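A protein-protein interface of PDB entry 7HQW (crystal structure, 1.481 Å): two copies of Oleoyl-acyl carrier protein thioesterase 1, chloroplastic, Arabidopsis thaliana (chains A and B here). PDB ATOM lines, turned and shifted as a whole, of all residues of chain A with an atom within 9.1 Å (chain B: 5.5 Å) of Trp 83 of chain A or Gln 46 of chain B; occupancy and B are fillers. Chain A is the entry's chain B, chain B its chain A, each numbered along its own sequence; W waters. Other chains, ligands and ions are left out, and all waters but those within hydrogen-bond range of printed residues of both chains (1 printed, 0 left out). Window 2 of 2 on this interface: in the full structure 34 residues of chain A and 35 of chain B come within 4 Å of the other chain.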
ATOM      1  N   PHE A  15     -18.305  -2.887  25.111  1.00  0.00           N
ATOM      2  CA  PHE A  15     -17.602  -1.593  25.044  1.00  0.00           C
ATOM      3  C   PHE A  15     -18.582  -0.471  25.310  1.00  0.00           C
ATOM      4  O   PHE A  15     -19.681  -0.494  24.761  1.00  0.00           O
ATOM      5  CB  PHE A  15     -17.007  -1.356  23.636  1.00  0.00           C
ATOM      6  CG  PHE A  15     -16.025  -2.419  23.217  1.00  0.00           C
ATOM      7  CD1 PHE A  15     -14.699  -2.347  23.598  1.00  0.00           C
ATOM      8  CD2 PHE A  15     -16.429  -3.490  22.436  1.00  0.00           C
ATOM      9  CE1 PHE A  15     -13.799  -3.340  23.223  1.00  0.00           C
ATOM     10  CE2 PHE A  15     -15.518  -4.444  22.011  1.00  0.00           C
ATOM     11  CZ  PHE A  15     -14.209  -4.372  22.410  1.00  0.00           C
ATOM     12  N   VAL A  16     -18.181   0.542  26.111  1.00  0.00           N
ATOM     13  CA  VAL A  16     -19.037   1.697  26.328  1.00  0.00           C
ATOM     14  C   VAL A  16     -18.576   2.767  25.327  1.00  0.00           C
ATOM     15  O   VAL A  16     -17.388   3.119  25.339  1.00  0.00           O
ATOM     16  CB  VAL A  16     -18.912   2.251  27.767  1.00  0.00           C
ATOM     17  CG1 VAL A  16     -19.793   3.486  27.932  1.00  0.00           C
ATOM     18  CG2 VAL A  16     -19.290   1.185  28.799  1.00  0.00           C
ATOM     19  N   VAL A  17     -19.467   3.277  24.475  1.00  0.00           N
ATOM     20  CA  VAL A  17     -19.074   4.301  23.477  1.00  0.00           C
ATOM     21  C   VAL A  17     -18.571   5.618  24.146  1.00  0.00           C
ATOM     22  O   VAL A  17     -19.267   6.199  24.982  1.00  0.00           O
ATOM     23  CB  VAL A  17     -20.199   4.547  22.445  1.00  0.00           C
ATOM     24  CG1 VAL A  17     -19.772   5.598  21.404  1.00  0.00           C
ATOM     25  CG2 VAL A  17     -20.577   3.225  21.757  1.00  0.00           C
ATOM     26  N   ARG A  18     -17.363   6.067  23.773  1.00  0.00           N
ATOM     27  CA  ARG A  18     -16.713   7.247  24.369  1.00  0.00           C
ATOM     28  C   ARG A  18     -17.077   8.574  23.658  1.00  0.00           C
ATOM     29  O   ARG A  18     -17.400   8.576  22.473  1.00  0.00           O
ATOM     30  CB  ARG A  18     -15.170   7.057  24.340  1.00  0.00           C
ATOM     31  CG  ARG A  18     -14.708   5.919  25.231  1.00  0.00           C
ATOM     32  CD  ARG A  18     -13.234   5.622  25.063  1.00  0.00           C
ATOM     33  NE  ARG A  18     -12.834   4.523  25.936  1.00  0.00           N
ATOM     34  CZ  ARG A  18     -11.629   3.948  25.911  1.00  0.00           C
ATOM     35  NH1 ARG A  18     -10.704   4.368  25.060  1.00  0.00           N
ATOM     36  NH2 ARG A  18     -11.348   2.947  26.730  1.00  0.00           N
ATOM     37  N   SER A  19     -16.930   9.710  24.362  1.00  0.00           N
ATOM     38  CA  SER A  19     -17.242  11.050  23.836  1.00  0.00           C
ATOM     39  C   SER A  19     -16.494  11.379  22.534  1.00  0.00           C
ATOM     40  O   SER A  19     -17.076  11.970  21.615  1.00  0.00           O
ATOM     41  CB  SER A  19     -16.897  12.130  24.869  1.00  0.00           C
ATOM     42  OG  SER A  19     -15.503  12.093  25.133  1.00  0.00           O
ATOM     43  N   TYR A  20     -15.189  11.024  22.452  1.00  0.00           N
ATOM     44  CA  TYR A  20     -14.420  11.354  21.244  1.00  0.00           C
ATOM     45  C   TYR A  20     -14.641  10.338  20.103  1.00  0.00           C
ATOM     46  O   TYR A  20     -14.115  10.523  18.998  1.00  0.00           O
ATOM     47  CB  TYR A  20     -12.938  11.556  21.597  1.00  0.00           C
ATOM     48  CG  TYR A  20     -12.263  10.302  22.123  1.00  0.00           C
ATOM     49  CD1 TYR A  20     -11.683   9.385  21.258  1.00  0.00           C
ATOM     50  CD2 TYR A  20     -12.199  10.036  23.489  1.00  0.00           C
ATOM     51  CE1 TYR A  20     -11.057   8.233  21.733  1.00  0.00           C
ATOM     52  CE2 TYR A  20     -11.583   8.878  23.978  1.00  0.00           C
ATOM     53  CZ  TYR A  20     -11.011   7.979  23.091  1.00  0.00           C
ATOM     54  OH  TYR A  20     -10.401   6.829  23.533  1.00  0.00           O
ATOM     55  N   GLU A  21     -15.424   9.283  20.347  1.00  0.00           N
ATOM     56  CA  GLU A  21     -15.660   8.224  19.355  1.00  0.00           C
ATOM     57  C   GLU A  21     -16.879   8.468  18.452  1.00  0.00           C
ATOM     58  O   GLU A  21     -17.112   7.649  17.551  1.00  0.00           O
ATOM     59  CB  GLU A  21     -15.884   6.879  20.096  1.00  0.00           C
ATOM     60  CG  GLU A  21     -14.582   6.229  20.554  1.00  0.00           C
ATOM     61  CD  GLU A  21     -14.707   4.959  21.385  1.00  0.00           C
ATOM     62  OE1 GLU A  21     -15.829   4.635  21.835  1.00  0.00           O
ATOM     63  OE2 GLU A  21     -13.673   4.284  21.592  1.00  0.00           O
ATOM     64  N   VAL A  22     -17.666   9.546  18.725  1.00  0.00           N
ATOM     65  CA  VAL A  22     -18.908   9.829  18.013  1.00  0.00           C
ATOM     66  C   VAL A  22     -18.802  10.959  16.983  1.00  0.00           C
ATOM     67  O   VAL A  22     -17.929  11.830  17.089  1.00  0.00           O
ATOM     68  CB  VAL A  22     -20.080  10.093  18.993  1.00  0.00           C
ATOM     69  CG1 VAL A  22     -20.197   8.969  20.033  1.00  0.00           C
ATOM     70  CG2 VAL A  22     -19.936  11.456  19.665  1.00  0.00           C
ATOM     71  N   GLY A  23     -19.696  10.913  15.998  1.00  0.00           N
ATOM     72  CA  GLY A  23     -19.788  11.915  14.931  1.00  0.00           C
ATOM     73  C   GLY A  23     -20.873  12.945  15.225  1.00  0.00           C
ATOM     74  O   GLY A  23     -21.326  13.067  16.363  1.00  0.00           O
ATOM     75  N   ASN A  25     -24.039  13.049  14.743  1.00  0.00           N
ATOM     76  CA  ASN A  25     -25.306  12.517  15.278  1.00  0.00           C
ATOM     77  C   ASN A  25     -25.184  12.023  16.752  1.00  0.00           C
ATOM     78  O   ASN A  25     -26.120  11.409  17.269  1.00  0.00           O
ATOM     79  CB  ASN A  25     -25.851  11.352  14.402  1.00  0.00           C
ATOM     80  CG  ASN A  25     -24.837  10.640  13.519  1.00  0.00           C
ATOM     81  OD1 ASN A  25     -23.954   9.891  13.999  1.00  0.00           O
ATOM     82  ND2 ASN A  25     -24.948  10.858  12.212  1.00  0.00           N
ATOM     83  N   LYS A  26     -24.022  12.251  17.400  1.00  0.00           N
ATOM     84  CA  LYS A  26     -23.732  11.757  18.750  1.00  0.00           C
ATOM     85  C   LYS A  26     -23.802  10.224  18.832  1.00  0.00           C
ATOM     86  O   LYS A  26     -24.081   9.672  19.895  1.00  0.00           O
ATOM     87  CB  LYS A  26     -24.586  12.413  19.844  1.00  0.00           C
ATOM     88  CG  LYS A  26     -24.569  13.924  19.818  1.00  0.00           C
ATOM     89  CD  LYS A  26     -25.587  14.464  20.822  1.00  0.00           C
ATOM     90  CE  LYS A  26     -25.919  15.911  20.576  1.00  0.00           C
ATOM     91  NZ  LYS A  26     -27.015  16.368  21.468  1.00  0.00           N
ATOM     92  N   THR A  27     -23.533   9.527  17.702  1.00  0.00           N
ATOM     93  CA  THR A  27     -23.452   8.073  17.693  1.00  0.00           C
ATOM     94  C   THR A  27     -22.055   7.679  17.147  1.00  0.00           C
ATOM     95  O   THR A  27     -21.396   8.475  16.464  1.00  0.00           O
ATOM     96  CB  THR A  27     -24.551   7.416  16.839  1.00  0.00           C
ATOM     97  OG1 THR A  27     -24.406   7.846  15.490  1.00  0.00           O
ATOM     98  CG2 THR A  27     -25.959   7.699  17.359  1.00  0.00           C
ATOM     99  N   ALA A  28     -21.623   6.463  17.444  1.00  0.00           N
ATOM    100  CA  ALA A  28     -20.307   5.964  17.037  1.00  0.00           C
ATOM    101  C   ALA A  28     -20.065   6.086  15.525  1.00  0.00           C
ATOM    102  O   ALA A  28     -20.982   5.782  14.752  1.00  0.00           O
ATOM    103  CB  ALA A  28     -20.156   4.510  17.462  1.00  0.00           C
ATOM    104  N   THR A  29     -18.860   6.527  15.091  1.00  0.00           N
ATOM    105  CA  THR A  29     -18.558   6.564  13.663  1.00  0.00           C
ATOM    106  C   THR A  29     -18.288   5.123  13.142  1.00  0.00           C
ATOM    107  O   THR A  29     -18.022   4.206  13.942  1.00  0.00           O
ATOM    108  CB  THR A  29     -17.318   7.442  13.400  1.00  0.00           C
ATOM    109  OG1 THR A  29     -16.158   6.864  14.018  1.00  0.00           O
ATOM    110  CG2 THR A  29     -17.507   8.900  13.830  1.00  0.00           C
ATOM    111  N   TYR A  80     -26.250   2.720  14.757  1.00  0.00           N
ATOM    112  CA  TYR A  80     -24.966   3.049  15.375  1.00  0.00           C
ATOM    113  C   TYR A  80     -25.238   3.315  16.856  1.00  0.00           C
ATOM    114  O   TYR A  80     -26.145   4.078  17.184  1.00  0.00           O
ATOM    115  CB  TYR A  80     -24.326   4.293  14.741  1.00  0.00           C
ATOM    116  CG  TYR A  80     -23.782   4.027  13.360  1.00  0.00           C
ATOM    117  CD1 TYR A  80     -22.494   3.550  13.180  1.00  0.00           C
ATOM    118  CD2 TYR A  80     -24.571   4.222  12.231  1.00  0.00           C
ATOM    119  CE1 TYR A  80     -21.991   3.296  11.907  1.00  0.00           C
ATOM    120  CE2 TYR A  80     -24.078   3.981  10.951  1.00  0.00           C
ATOM    121  CZ  TYR A  80     -22.780   3.528  10.790  1.00  0.00           C
ATOM    122  OH  TYR A  80     -22.257   3.263   9.531  1.00  0.00           O
ATOM    123  N   PRO A  81     -24.399   2.778  17.747  1.00  0.00           N
ATOM    124  CA  PRO A  81     -24.631   3.001  19.186  1.00  0.00           C
ATOM    125  C   PRO A  81     -24.355   4.446  19.568  1.00  0.00           C
ATOM    126  O   PRO A  81     -23.400   5.047  19.086  1.00  0.00           O
ATOM    127  CB  PRO A  81     -23.642   2.031  19.867  1.00  0.00           C
ATOM    128  CG  PRO A  81     -22.557   1.828  18.864  1.00  0.00           C
ATOM    129  CD  PRO A  81     -23.262   1.862  17.506  1.00  0.00           C
ATOM    130  N   ALA A  82     -25.182   5.000  20.431  1.00  0.00           N
ATOM    131  CA  ALA A  82     -25.021   6.381  20.871  1.00  0.00           C
ATOM    132  C   ALA A  82     -23.897   6.503  21.917  1.00  0.00           C
ATOM    133  O   ALA A  82     -23.496   5.515  22.551  1.00  0.00           O
ATOM    134  CB  ALA A  82     -26.353   6.894  21.444  1.00  0.00           C
ATOM    135  N   TRP A  83     -23.411   7.732  22.160  1.00  0.00           N
ATOM    136  CA  TRP A  83     -22.436   7.975  23.220  1.00  0.00           C
ATOM    137  C   TRP A  83     -22.994   7.461  24.591  1.00  0.00           C
ATOM    138  O   TRP A  83     -24.156   7.719  24.916  1.00  0.00           O
ATOM    139  CB  TRP A  83     -22.140   9.470  23.276  1.00  0.00           C
ATOM    140  CG  TRP A  83     -21.538   9.919  24.564  1.00  0.00           C
ATOM    141  CD1 TRP A  83     -20.272   9.688  24.997  1.00  0.00           C
ATOM    142  CD2 TRP A  83     -22.216  10.594  25.632  1.00  0.00           C
ATOM    143  NE1 TRP A  83     -20.099  10.218  26.253  1.00  0.00           N
ATOM    144  CE2 TRP A  83     -21.284  10.766  26.674  1.00  0.00           C
ATOM    145  CE3 TRP A  83     -23.530  11.046  25.820  1.00  0.00           C
ATOM    146  CZ2 TRP A  83     -21.609  11.418  27.865  1.00  0.00           C
ATOM    147  CZ3 TRP A  83     -23.845  11.693  26.998  1.00  0.00           C
ATOM    148  CH2 TRP A  83     -22.889  11.877  28.000  1.00  0.00           C
ATOM    149  N   GLY A  84     -22.180   6.699  25.316  1.00  0.00           N
ATOM    150  CA  GLY A  84     -22.573   6.126  26.605  1.00  0.00           C
ATOM    151  C   GLY A  84     -23.283   4.783  26.524  1.00  0.00           C
ATOM    152  O   GLY A  84     -23.482   4.126  27.556  1.00  0.00           O
ATOM    153  N   ASP A  85     -23.703   4.370  25.319  1.00  0.00           N
ATOM    154  CA  ASP A  85     -24.356   3.071  25.126  1.00  0.00           C
ATOM    155  C   ASP A  85     -23.337   1.931  25.234  1.00  0.00           C
ATOM    156  O   ASP A  85     -22.148   2.126  24.958  1.00  0.00           O
ATOM    157  CB  ASP A  85     -25.015   2.983  23.742  1.00  0.00           C
ATOM    158  CG  ASP A  85     -26.356   3.691  23.621  1.00  0.00           C
ATOM    159  OD1 ASP A  85     -26.798   4.302  24.621  1.00  0.00           O
ATOM    160  OD2 ASP A  85     -26.959   3.641  22.515  1.00  0.00           O
ATOM    161  N   VAL A  86     -23.805   0.741  25.649  1.00  0.00           N
ATOM    162  CA  VAL A  86     -22.912  -0.417  25.739  1.00  0.00           C
ATOM    163  C   VAL A  86     -23.221  -1.321  24.532  1.00  0.00           C
ATOM    164  O   VAL A  86     -24.380  -1.713  24.340  1.00  0.00           O
ATOM    165  CB  VAL A  86     -23.131  -1.185  27.069  1.00  0.00           C
ATOM    166  CG1 VAL A  86     -22.179  -2.386  27.179  1.00  0.00           C
ATOM    167  CG2 VAL A  86     -22.994  -0.251  28.274  1.00  0.00           C
ATOM    168  N   GLU B  39     -12.032  12.200  27.917  1.00  0.00           N
ATOM    169  CA  GLU B  39     -13.127  11.296  28.235  1.00  0.00           C
ATOM    170  C   GLU B  39     -13.565  11.420  29.699  1.00  0.00           C
ATOM    171  O   GLU B  39     -14.756  11.613  29.962  1.00  0.00           O
ATOM    172  CB  GLU B  39     -12.796   9.848  27.857  1.00  0.00           C
ATOM    173  CG  GLU B  39     -13.857   8.818  28.261  1.00  0.00           C
ATOM    174  CD  GLU B  39     -15.184   8.931  27.533  1.00  0.00           C
ATOM    175  OE1 GLU B  39     -15.309   9.817  26.658  1.00  0.00           O
ATOM    176  OE2 GLU B  39     -16.103   8.145  27.848  1.00  0.00           O
ATOM    177  N   GLY B  41     -12.969  13.941  31.702  1.00  0.00           N
ATOM    178  CA  GLY B  41     -13.482  15.299  31.920  1.00  0.00           C
ATOM    179  C   GLY B  41     -14.947  15.371  31.497  1.00  0.00           C
ATOM    180  O   GLY B  41     -15.758  15.976  32.204  1.00  0.00           O
ATOM    181  N   CYS B  42     -15.292  14.722  30.375  1.00  0.00           N
ATOM    182  CA  CYS B  42     -16.658  14.690  29.865  1.00  0.00           C
ATOM    183  C   CYS B  42     -17.585  13.923  30.804  1.00  0.00           C
ATOM    184  O   CYS B  42     -18.721  14.347  31.040  1.00  0.00           O
ATOM    185  CB  CYS B  42     -16.696  14.105  28.460  1.00  0.00           C
ATOM    186  SG  CYS B  42     -18.314  14.224  27.672  1.00  0.00           S
ATOM    187  N   ASN B  43     -17.115  12.784  31.323  1.00  0.00           N
ATOM    188  CA  ASN B  43     -17.926  11.962  32.251  1.00  0.00           C
ATOM    189  C   ASN B  43     -18.153  12.699  33.573  1.00  0.00           C
ATOM    190  O   ASN B  43     -19.235  12.599  34.167  1.00  0.00           O
ATOM    191  CB  ASN B  43     -17.330  10.543  32.429  1.00  0.00           C
ATOM    192  CG  ASN B  43     -17.512   9.733  31.145  1.00  0.00           C
ATOM    193  OD1 ASN B  43     -18.464   9.965  30.371  1.00  0.00           O
ATOM    194  ND2 ASN B  43     -16.629   8.774  30.877  1.00  0.00           N
ATOM    195  N   HIS B  44     -17.172  13.504  33.992  1.00  0.00           N
ATOM    196  CA  HIS B  44     -17.319  14.309  35.193  1.00  0.00           C
ATOM    197  C   HIS B  44     -18.431  15.391  34.971  1.00  0.00           C
ATOM    198  O   HIS B  44     -19.343  15.527  35.801  1.00  0.00           O
ATOM    199  CB  HIS B  44     -15.994  15.003  35.525  1.00  0.00           C
ATOM    200  CG  HIS B  44     -16.001  15.763  36.810  1.00  0.00           C
ATOM    201  ND1 HIS B  44     -14.964  16.640  37.126  1.00  0.00           N
ATOM    202  CD2 HIS B  44     -16.890  15.732  37.846  1.00  0.00           C
ATOM    203  CE1 HIS B  44     -15.256  17.112  38.331  1.00  0.00           C
ATOM    204  NE2 HIS B  44     -16.419  16.620  38.793  1.00  0.00           N
ATOM    205  N   ALA B  45     -18.393  16.109  33.826  1.00  0.00           N
ATOM    206  CA  ALA B  45     -19.456  17.073  33.489  1.00  0.00           C
ATOM    207  C   ALA B  45     -20.853  16.379  33.482  1.00  0.00           C
ATOM    208  O   ALA B  45     -21.803  16.915  34.049  1.00  0.00           O
ATOM    209  CB  ALA B  45     -19.181  17.699  32.114  1.00  0.00           C
ATOM    210  N   GLN B  46     -20.961  15.194  32.844  1.00  0.00           N
ATOM    211  CA  GLN B  46     -22.213  14.445  32.750  1.00  0.00           C
ATOM    212  C   GLN B  46     -22.751  14.127  34.154  1.00  0.00           C
ATOM    213  O   GLN B  46     -23.959  14.244  34.425  1.00  0.00           O
ATOM    214  CB  GLN B  46     -22.012  13.114  31.975  1.00  0.00           C
ATOM    215  CG  GLN B  46     -23.329  12.421  31.558  1.00  0.00           C
ATOM    216  CD  GLN B  46     -24.064  11.608  32.614  1.00  0.00           C
ATOM    217  OE1 GLN B  46     -25.306  11.547  32.623  1.00  0.00           O
ATOM    218  NE2 GLN B  46     -23.342  10.972  33.532  1.00  0.00           N
ATOM    219  N   SER B  47     -21.854  13.702  35.033  1.00  0.00           N
ATOM    220  CA  SER B  47     -22.226  13.262  36.382  1.00  0.00           C
ATOM    221  C   SER B  47     -22.924  14.339  37.212  1.00  0.00           C
ATOM    222  O   SER B  47     -23.680  14.002  38.129  1.00  0.00           O
ATOM    223  CB  SER B  47     -20.999  12.735  37.123  1.00  0.00           C
ATOM    224  OG  SER B  47     -20.184  13.768  37.656  1.00  0.00           O
ATOM    225  N   VAL B  48     -22.669  15.628  36.897  1.00  0.00           N
ATOM    226  CA  VAL B  48     -23.266  16.750  37.649  1.00  0.00           C
ATOM    227  C   VAL B  48     -24.227  17.646  36.828  1.00  0.00           C
ATOM    228  O   VAL B  48     -24.716  18.648  37.360  1.00  0.00           O
ATOM    229  CB  VAL B  48     -22.208  17.609  38.368  1.00  0.00           C
ATOM    230  CG1 VAL B  48     -21.452  16.788  39.412  1.00  0.00           C
ATOM    231  CG2 VAL B  48     -21.248  18.240  37.366  1.00  0.00           C
ATOM    232  N   GLY B  49     -24.526  17.280  35.569  1.00  0.00           N
ATOM    233  CA  GLY B  49     -25.540  17.998  34.797  1.00  0.00           C
ATOM    234  C   GLY B  49     -25.088  19.050  33.793  1.00  0.00           C
ATOM    235  O   GLY B  49     -25.939  19.766  33.245  1.00  0.00           O
ATOM    236  N   PHE B  50     -23.764  19.199  33.584  1.00  0.00           N
ATOM    237  CA  PHE B  50     -23.267  20.188  32.617  1.00  0.00           C
ATOM    238  C   PHE B  50     -23.288  19.586  31.201  1.00  0.00           C
ATOM    239  O   PHE B  50     -23.447  18.362  31.065  1.00  0.00           O
ATOM    240  CB  PHE B  50     -21.858  20.669  33.002  1.00  0.00           C
ATOM    241  CG  PHE B  50     -21.829  21.479  34.271  1.00  0.00           C
ATOM    242  CD1 PHE B  50     -22.709  22.525  34.463  1.00  0.00           C
ATOM    243  CD2 PHE B  50     -20.966  21.148  35.302  1.00  0.00           C
ATOM    244  CE1 PHE B  50     -22.707  23.244  35.656  1.00  0.00           C
ATOM    245  CE2 PHE B  50     -20.966  21.866  36.487  1.00  0.00           C
ATOM    246  CZ  PHE B  50     -21.845  22.901  36.663  1.00  0.00           C
ATOM    247  N   SER B  51     -23.064  20.430  30.129  1.00  0.00           N
ATOM    248  CA  SER B  51     -23.045  19.871  28.779  1.00  0.00           C
ATOM    249  C   SER B  51     -21.973  18.791  28.616  1.00  0.00           C
ATOM    250  O   SER B  51     -20.976  18.772  29.343  1.00  0.00           O
ATOM    251  CB  SER B  51     -22.881  20.954  27.713  1.00  0.00           C
ATOM    252  OG  SER B  51     -21.544  21.435  27.634  1.00  0.00           O
ATOM    253  N   THR B  52     -22.218  17.850  27.707  1.00  0.00           N
ATOM    254  CA  THR B  52     -21.263  16.768  27.454  1.00  0.00           C
ATOM    255  C   THR B  52     -20.683  16.860  26.051  1.00  0.00           C
ATOM    256  O   THR B  52     -20.501  15.845  25.373  1.00  0.00           O
ATOM    257  CB  THR B  52     -21.945  15.443  27.714  1.00  0.00           C
ATOM    258  OG1 THR B  52     -23.124  15.352  26.896  1.00  0.00           O
ATOM    259  CG2 THR B  52     -22.351  15.311  29.184  1.00  0.00           C
HETATM  260  O   HOH W   1     -19.256   7.064  27.554  1.00  0.00           O
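OE2 of Glu 39 of chain B lies within hydrogen-bond range of ND2 of Asn 43 of chain B, at 3.1 Å.
The side-chain sulfur (SG) of Cys 42 of chain B sits at hydrogen-bond distance from the backbone carbonyl oxygen (O) of Thr 52 of chain B (3.6 Å).
The side-chain hydroxyl of Tyr 20 of chain A sits at hydrogen-bond distance from the guanidinium group of Arg 18 of chain A (2.9 Å).
The side-chain carboxylate of Glu 21 of chain A lies within hydrogen-bond range of the backbone NH of Arg 18 of chain A.
O of Lys 26 of chain A sits at hydrogen-bond distance from N of Trp 83 of chain A, 3.1 Å away.
The side-chain carboxylate (OE1) of Glu 39 of chain B is in hydrogen-bond range of the side-chain hydroxyl (OG) of Ser 19 of chain A, 2.7 Å away.
Printed residues of chain B that touch a printed residue of chain A: Glu 39, Cys 42, Gln 46 and Thr 52.
Among the printed residues, 5 pairs touch across the chains.
Among the printed residues, no Asp or Glu carboxylate lies within 4 Å of a Lys or Arg side-chain nitrogen of the other chain.
Among the printed residues, merely in contact across the chains: Arg 18 of chain A with Glu 39 of chain B, Trp 83 of chain A with Gln 46 of chain B, Trp 83 of chain A with Thr 52 of chain B and Ser 19 of chain A with Cys 42 of chain B.
Of the printed residues of chain B, Arg 18 of chain A touches Glu 39.
Printed residues of chain B within 4 Å of Ser 19 of chain A: Glu 39 and Cys 42.
Tyr 80 of chain A touches none of the printed residues of chain B.
Of the printed residues of chain A, Glu 39 of chain B touches Arg 18 and Ser 19.
Ala 45 of chain B touches none of the printed residues of chain A.
Printed residues of chain A within 4 Å of Gln 46 of chain B: Trp 83.
Ser 47 of chain B touches none of the printed residues of chain A.
Printed residues of chain A within 4 Å of Thr 52 of chain B: Trp 83.
The nearest residue of chain B that does not touch Trp 83 of chain A is Asn 43 of chain B (4.3 Å).
Water W1 lies within hydrogen-bond range of O of Val 17 of chain A (2.7 Å) and OE2 of Glu 39 of chain B (3.3 Å).
No position is printed for both chains.
Of the 5 pairs that touch across the chains among the printed residues, none has its exchanged pair printed and touching as well.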
